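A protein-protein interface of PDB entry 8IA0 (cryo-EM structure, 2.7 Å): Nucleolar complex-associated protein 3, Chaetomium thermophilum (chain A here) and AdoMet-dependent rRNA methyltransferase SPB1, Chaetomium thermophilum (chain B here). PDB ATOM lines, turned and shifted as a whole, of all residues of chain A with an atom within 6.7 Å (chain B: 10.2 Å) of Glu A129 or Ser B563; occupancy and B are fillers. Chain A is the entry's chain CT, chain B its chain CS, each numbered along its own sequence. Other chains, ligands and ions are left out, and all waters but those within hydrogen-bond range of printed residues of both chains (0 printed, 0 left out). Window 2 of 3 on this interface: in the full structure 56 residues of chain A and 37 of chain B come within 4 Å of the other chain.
Among the printed residues, merely in contact across the chains: Gln A128 with Phe B570, Glu A129 with Ala B566, Leu A131 with Phe B570, Ala A132 with Ala B566 and Ala A132 with Phe B570.
Of the 11 printed residues of chain B, 4 touch a printed residue of chain A. Along chain B the printed residues that touch a printed residue of chain A span positions 563 to 570. Among the printed residues, no Asp or Glu carboxylate lies within 4 Å of a Lys or Arg side-chain nitrogen of the other chain.
Arg A125 touches none of the printed residues of chain B. No residue of chain B comes within 4 Å of Ala A127. Of the printed residues of chain B, Gln A128 touches Phe B570. Glu A129 touches two residues of chain B. Glu A130 touches none of the printed residues of chain B. Printed residues of chain B within 4 Å of Lys A133: Arg B565 (3.1 Å). Printed residues of chain A within 4 Å of Arg B565: Lys A133 (3.1 Å). Of the printed residues of chain A, Ala B566 touches Glu A129 and Ala A132. Arg B567 touches none of the printed residues of chain A. Of the printed residues of chain A, Phe B570 touches Gln A128 (3.3 Å), Leu A131 (3.4 Å) and Ala A132 (3.6 Å). The nearest residue of chain A that does not touch Ser B563 is Ala A132 (5.5 Å). The nearest printed residue of chain B that does not touch Lys A133 is Phe B570 (6.2 Å).
The side-chain amide nitrogen (NE2) of Gln A128 sits close to the backbone carbonyl oxygen (O) of Ile A124 (3.3 Å). The backbone NH (N) of Ala B566 lies within hydrogen-bond range of the side-chain hydroxyl (OG) of Ser B563, at 3.2 Å.
OG of Ser B563 lies within hydrogen-bond range of OE2 of Glu A129, at 3.0 Å. NZ of Lys A133 lies close to NH2 of Arg B565.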
ATOM      1  N   ILE A 124       2.917   9.885  15.730  1.00  0.00           N
ATOM      2  CA  ILE A 124       2.195   9.381  16.893  1.00  0.00           C
ATOM      3  C   ILE A 124       2.499   7.905  17.112  1.00  0.00           C
ATOM      4  O   ILE A 124       2.601   7.444  18.256  1.00  0.00           O
ATOM      5  CB  ILE A 124       0.682   9.639  16.752  1.00  0.00           C
ATOM      6  CG1 ILE A 124       0.171   9.166  15.393  1.00  0.00           C
ATOM      7  CG2 ILE A 124       0.367  11.113  16.956  1.00  0.00           C
ATOM      8  CD1 ILE A 124      -1.342   9.108  15.287  1.00  0.00           C
ATOM      9  N   ARG A 125       2.652   7.134  16.027  1.00  0.00           N
ATOM     10  CA  ARG A 125       3.008   5.727  16.196  1.00  0.00           C
ATOM     11  C   ARG A 125       4.378   5.606  16.843  1.00  0.00           C
ATOM     12  O   ARG A 125       4.578   4.783  17.745  1.00  0.00           O
ATOM     13  CB  ARG A 125       2.997   4.984  14.855  1.00  0.00           C
ATOM     14  CG  ARG A 125       4.084   3.898  14.748  1.00  0.00           C
ATOM     15  CD  ARG A 125       4.457   3.476  13.321  1.00  0.00           C
ATOM     16  NE  ARG A 125       4.490   4.556  12.343  1.00  0.00           N
ATOM     17  CZ  ARG A 125       5.416   5.506  12.309  1.00  0.00           C
ATOM     18  NH1 ARG A 125       6.415   5.532  13.171  1.00  0.00           N
ATOM     19  NH2 ARG A 125       5.346   6.446  11.373  1.00  0.00           N
ATOM     20  N   GLN A 126       5.325   6.437  16.407  1.00  0.00           N
ATOM     21  CA  GLN A 126       6.650   6.437  17.015  1.00  0.00           C
ATOM     22  C   GLN A 126       6.575   6.830  18.484  1.00  0.00           C
ATOM     23  O   GLN A 126       7.215   6.204  19.336  1.00  0.00           O
ATOM     24  CB  GLN A 126       7.571   7.384  16.248  1.00  0.00           C
ATOM     25  CG  GLN A 126       8.767   7.872  17.041  1.00  0.00           C
ATOM     26  CD  GLN A 126      10.051   7.799  16.243  1.00  0.00           C
ATOM     27  OE1 GLN A 126      10.087   7.217  15.158  1.00  0.00           O
ATOM     28  NE2 GLN A 126      11.115   8.382  16.778  1.00  0.00           N
ATOM     29  N   ALA A 127       5.783   7.857  18.800  1.00  0.00           N
ATOM     30  CA  ALA A 127       5.609   8.254  20.192  1.00  0.00           C
ATOM     31  C   ALA A 127       4.915   7.162  20.996  1.00  0.00           C
ATOM     32  O   ALA A 127       5.262   6.926  22.159  1.00  0.00           O
ATOM     33  CB  ALA A 127       4.823   9.561  20.271  1.00  0.00           C
ATOM     34  N   GLN A 128       3.927   6.494  20.398  1.00  0.00           N
ATOM     35  CA  GLN A 128       3.238   5.414  21.094  1.00  0.00           C
ATOM     36  C   GLN A 128       4.195   4.281  21.434  1.00  0.00           C
ATOM     37  O   GLN A 128       4.098   3.676  22.508  1.00  0.00           O
ATOM     38  CB  GLN A 128       2.081   4.895  20.242  1.00  0.00           C
ATOM     39  CG  GLN A 128       0.792   5.665  20.417  1.00  0.00           C
ATOM     40  CD  GLN A 128      -0.284   5.221  19.452  1.00  0.00           C
ATOM     41  OE1 GLN A 128      -1.329   4.717  19.859  1.00  0.00           O
ATOM     42  NE2 GLN A 128      -0.034   5.407  18.162  1.00  0.00           N
ATOM     43  N   GLU A 129       5.120   3.972  20.523  1.00  0.00           N
ATOM     44  CA  GLU A 129       6.092   2.917  20.782  1.00  0.00           C
ATOM     45  C   GLU A 129       6.980   3.267  21.968  1.00  0.00           C
ATOM     46  O   GLU A 129       7.282   2.407  22.802  1.00  0.00           O
ATOM     47  CB  GLU A 129       6.937   2.669  19.530  1.00  0.00           C
ATOM     48  CG  GLU A 129       6.372   1.691  18.475  1.00  0.00           C
ATOM     49  CD  GLU A 129       5.887   0.330  18.994  1.00  0.00           C
ATOM     50  OE1 GLU A 129       5.731  -0.575  18.148  1.00  0.00           O
ATOM     51  OE2 GLU A 129       5.679   0.130  20.209  1.00  0.00           O
ATOM     52  N   GLU A 130       7.415   4.526  22.054  1.00  0.00           N
ATOM     53  CA  GLU A 130       8.250   4.940  23.175  1.00  0.00           C
ATOM     54  C   GLU A 130       7.475   4.895  24.488  1.00  0.00           C
ATOM     55  O   GLU A 130       8.029   4.524  25.530  1.00  0.00           O
ATOM     56  CB  GLU A 130       8.809   6.337  22.920  1.00  0.00           C
ATOM     57  CG  GLU A 130      10.201   6.553  23.483  1.00  0.00           C
ATOM     58  CD  GLU A 130      11.247   5.697  22.794  1.00  0.00           C
ATOM     59  OE1 GLU A 130      11.390   5.805  21.558  1.00  0.00           O
ATOM     60  OE2 GLU A 130      11.926   4.915  23.492  1.00  0.00           O
ATOM     61  N   LEU A 131       6.198   5.284  24.461  1.00  0.00           N
ATOM     62  CA  LEU A 131       5.361   5.200  25.657  1.00  0.00           C
ATOM     63  C   LEU A 131       5.223   3.762  26.135  1.00  0.00           C
ATOM     64  O   LEU A 131       5.359   3.476  27.331  1.00  0.00           O
ATOM     65  CB  LEU A 131       3.986   5.801  25.374  1.00  0.00           C
ATOM     66  CG  LEU A 131       3.892   7.312  25.206  1.00  0.00           C
ATOM     67  CD1 LEU A 131       2.496   7.795  25.535  1.00  0.00           C
ATOM     68  CD2 LEU A 131       4.877   7.937  26.152  1.00  0.00           C
ATOM     69  N   ALA A 132       4.941   2.841  25.213  1.00  0.00           N
ATOM     70  CA  ALA A 132       4.827   1.436  25.584  1.00  0.00           C
ATOM     71  C   ALA A 132       6.155   0.901  26.094  1.00  0.00           C
ATOM     72  O   ALA A 132       6.194   0.104  27.038  1.00  0.00           O
ATOM     73  CB  ALA A 132       4.338   0.617  24.391  1.00  0.00           C
ATOM     74  N   LYS A 133       7.257   1.329  25.475  1.00  0.00           N
ATOM     75  CA  LYS A 133       8.577   0.885  25.902  1.00  0.00           C
ATOM     76  C   LYS A 133       8.861   1.296  27.340  1.00  0.00           C
ATOM     77  O   LYS A 133       9.211   0.460  28.178  1.00  0.00           O
ATOM     78  CB  LYS A 133       9.641   1.449  24.961  1.00  0.00           C
ATOM     79  CG  LYS A 133      11.055   1.379  25.509  1.00  0.00           C
ATOM     80  CD  LYS A 133      11.706   0.047  25.182  1.00  0.00           C
ATOM     81  CE  LYS A 133      12.386   0.086  23.824  1.00  0.00           C
ATOM     82  NZ  LYS A 133      13.158  -1.157  23.558  1.00  0.00           N
ATOM     83  N   ILE A 134       8.694   2.584  27.648  1.00  0.00           N
ATOM     84  CA  ILE A 134       9.083   3.093  28.960  1.00  0.00           C
ATOM     85  C   ILE A 134       8.206   2.490  30.050  1.00  0.00           C
ATOM     86  O   ILE A 134       8.698   2.044  31.094  1.00  0.00           O
ATOM     87  CB  ILE A 134       9.022   4.630  28.980  1.00  0.00           C
ATOM     88  CG1 ILE A 134      10.290   5.226  28.374  1.00  0.00           C
ATOM     89  CG2 ILE A 134       8.855   5.131  30.399  1.00  0.00           C
ATOM     90  CD1 ILE A 134      10.083   6.591  27.759  1.00  0.00           C
ATOM     91  N   GLN B 424      15.618 -12.949  20.669  1.00  0.00           N
ATOM     92  CA  GLN B 424      15.619 -12.106  19.473  1.00  0.00           C
ATOM     93  C   GLN B 424      16.622 -10.960  19.612  1.00  0.00           C
ATOM     94  O   GLN B 424      16.276  -9.779  19.551  1.00  0.00           O
ATOM     95  CB  GLN B 424      14.213 -11.575  19.174  1.00  0.00           C
ATOM     96  CG  GLN B 424      13.416 -12.430  18.212  1.00  0.00           C
ATOM     97  CD  GLN B 424      11.941 -12.088  18.228  1.00  0.00           C
ATOM     98  OE1 GLN B 424      11.479 -11.327  19.078  1.00  0.00           O
ATOM     99  NE2 GLN B 424      11.195 -12.640  17.280  1.00  0.00           N
ATOM    100  N   ASP B 551       4.896 -16.875  22.692  1.00  0.00           N
ATOM    101  CA  ASP B 551       3.575 -16.833  23.300  1.00  0.00           C
ATOM    102  C   ASP B 551       2.515 -16.909  22.211  1.00  0.00           C
ATOM    103  O   ASP B 551       2.506 -16.093  21.284  1.00  0.00           O
ATOM    104  CB  ASP B 551       3.406 -15.559  24.127  1.00  0.00           C
ATOM    105  CG  ASP B 551       3.938 -14.329  23.417  1.00  0.00           C
ATOM    106  OD1 ASP B 551       4.640 -14.487  22.396  1.00  0.00           O
ATOM    107  OD2 ASP B 551       3.655 -13.204  23.880  1.00  0.00           O
ATOM    108  N   SER B 563       3.394  -2.845  17.685  1.00  0.00           N
ATOM    109  CA  SER B 563       4.006  -4.023  18.283  1.00  0.00           C
ATOM    110  C   SER B 563       3.053  -4.691  19.263  1.00  0.00           C
ATOM    111  O   SER B 563       2.034  -4.114  19.637  1.00  0.00           O
ATOM    112  CB  SER B 563       5.311  -3.653  18.989  1.00  0.00           C
ATOM    113  OG  SER B 563       5.063  -2.843  20.123  1.00  0.00           O
ATOM    114  N   LYS B 564       3.390  -5.914  19.676  1.00  0.00           N
ATOM    115  CA  LYS B 564       2.524  -6.654  20.586  1.00  0.00           C
ATOM    116  C   LYS B 564       2.403  -5.946  21.931  1.00  0.00           C
ATOM    117  O   LYS B 564       1.307  -5.843  22.494  1.00  0.00           O
ATOM    118  CB  LYS B 564       3.051  -8.076  20.772  1.00  0.00           C
ATOM    119  CG  LYS B 564       2.046  -9.030  21.397  1.00  0.00           C
ATOM    120  CD  LYS B 564       2.738 -10.205  22.067  1.00  0.00           C
ATOM    121  CE  LYS B 564       3.634 -10.951  21.092  1.00  0.00           C
ATOM    122  NZ  LYS B 564       2.913 -11.315  19.841  1.00  0.00           N
ATOM    123  N   ARG B 565       3.522  -5.450  22.462  1.00  0.00           N
ATOM    124  CA  ARG B 565       3.476  -4.775  23.755  1.00  0.00           C
ATOM    125  C   ARG B 565       2.801  -3.413  23.657  1.00  0.00           C
ATOM    126  O   ARG B 565       2.187  -2.960  24.630  1.00  0.00           O
ATOM    127  CB  ARG B 565       4.886  -4.636  24.333  1.00  0.00           C
ATOM    128  CG  ARG B 565       5.780  -3.648  23.606  1.00  0.00           C
ATOM    129  CD  ARG B 565       7.006  -3.313  24.435  1.00  0.00           C
ATOM    130  NE  ARG B 565       8.146  -2.956  23.601  1.00  0.00           N
ATOM    131  CZ  ARG B 565       9.381  -2.792  24.054  1.00  0.00           C
ATOM    132  NH1 ARG B 565       9.673  -2.943  25.335  1.00  0.00           N
ATOM    133  NH2 ARG B 565      10.347  -2.468  23.200  1.00  0.00           N
ATOM    134  N   ALA B 566       2.904  -2.748  22.505  1.00  0.00           N
ATOM    135  CA  ALA B 566       2.237  -1.462  22.335  1.00  0.00           C
ATOM    136  C   ALA B 566       0.724  -1.626  22.361  1.00  0.00           C
ATOM    137  O   ALA B 566       0.023  -0.920  23.094  1.00  0.00           O
ATOM    138  CB  ALA B 566       2.685  -0.805  21.030  1.00  0.00           C
ATOM    139  N   ARG B 567       0.200  -2.559  21.567  1.00  0.00           N
ATOM    140  CA  ARG B 567      -1.237  -2.796  21.568  1.00  0.00           C
ATOM    141  C   ARG B 567      -1.697  -3.341  22.914  1.00  0.00           C
ATOM    142  O   ARG B 567      -2.834  -3.103  23.333  1.00  0.00           O
ATOM    143  CB  ARG B 567      -1.614  -3.752  20.435  1.00  0.00           C
ATOM    144  CG  ARG B 567      -1.845  -3.062  19.095  1.00  0.00           C
ATOM    145  CD  ARG B 567      -0.586  -3.092  18.241  1.00  0.00           C
ATOM    146  NE  ARG B 567      -0.821  -2.628  16.878  1.00  0.00           N
ATOM    147  CZ  ARG B 567      -0.461  -1.437  16.419  1.00  0.00           C
ATOM    148  NH1 ARG B 567       0.156  -0.557  17.191  1.00  0.00           N
ATOM    149  NH2 ARG B 567      -0.722  -1.123  15.154  1.00  0.00           N
ATOM    150  N   GLY B 568      -0.825  -4.078  23.602  1.00  0.00           N
ATOM    151  CA  GLY B 568      -1.171  -4.578  24.921  1.00  0.00           C
ATOM    152  C   GLY B 568      -1.282  -3.490  25.970  1.00  0.00           C
ATOM    153  O   GLY B 568      -2.153  -3.551  26.842  1.00  0.00           O
ATOM    154  N   PHE B 569      -0.409  -2.485  25.908  1.00  0.00           N
ATOM    155  CA  PHE B 569      -0.403  -1.458  26.945  1.00  0.00           C
ATOM    156  C   PHE B 569      -1.386  -0.333  26.647  1.00  0.00           C
ATOM    157  O   PHE B 569      -1.835   0.357  27.568  1.00  0.00           O
ATOM    158  CB  PHE B 569       1.002  -0.886  27.124  1.00  0.00           C
ATOM    159  CG  PHE B 569       1.064   0.231  28.120  1.00  0.00           C
ATOM    160  CD1 PHE B 569       0.784  -0.002  29.456  1.00  0.00           C
ATOM    161  CD2 PHE B 569       1.369   1.519  27.720  1.00  0.00           C
ATOM    162  CE1 PHE B 569       0.828   1.023  30.376  1.00  0.00           C
ATOM    163  CE2 PHE B 569       1.413   2.549  28.635  1.00  0.00           C
ATOM    164  CZ  PHE B 569       1.139   2.302  29.965  1.00  0.00           C
ATOM    165  N   PHE B 570      -1.724  -0.117  25.383  1.00  0.00           N
ATOM    166  CA  PHE B 570      -2.663   0.939  25.029  1.00  0.00           C
ATOM    167  C   PHE B 570      -4.090   0.437  24.865  1.00  0.00           C
ATOM    168  O   PHE B 570      -4.954   1.207  24.434  1.00  0.00           O
ATOM    169  CB  PHE B 570      -2.211   1.654  23.755  1.00  0.00           C
ATOM    170  CG  PHE B 570      -0.991   2.507  23.944  1.00  0.00           C
ATOM    171  CD1 PHE B 570       0.271   1.945  23.979  1.00  0.00           C
ATOM    172  CD2 PHE B 570      -1.112   3.876  24.089  1.00  0.00           C
ATOM    173  CE1 PHE B 570       1.388   2.730  24.153  1.00  0.00           C
ATOM    174  CE2 PHE B 570       0.001   4.667  24.264  1.00  0.00           C
ATOM    175  CZ  PHE B 570       1.252   4.093  24.295  1.00  0.00           C
ATOM    176  N   SER B 571      -4.359  -0.825  25.195  1.00  0.00           N
ATOM    177  CA  SER B 571      -5.713  -1.362  25.189  1.00  0.00           C
ATOM    178  C   SER B 571      -6.236  -1.616  26.599  1.00  0.00           C
ATOM    179  O   SER B 571      -7.088  -2.489  26.797  1.00  0.00           O
ATOM    180  CB  SER B 571      -5.775  -2.646  24.363  1.00  0.00           C
ATOM    181  OG  SER B 571      -5.001  -3.673  24.957  1.00  0.00           O
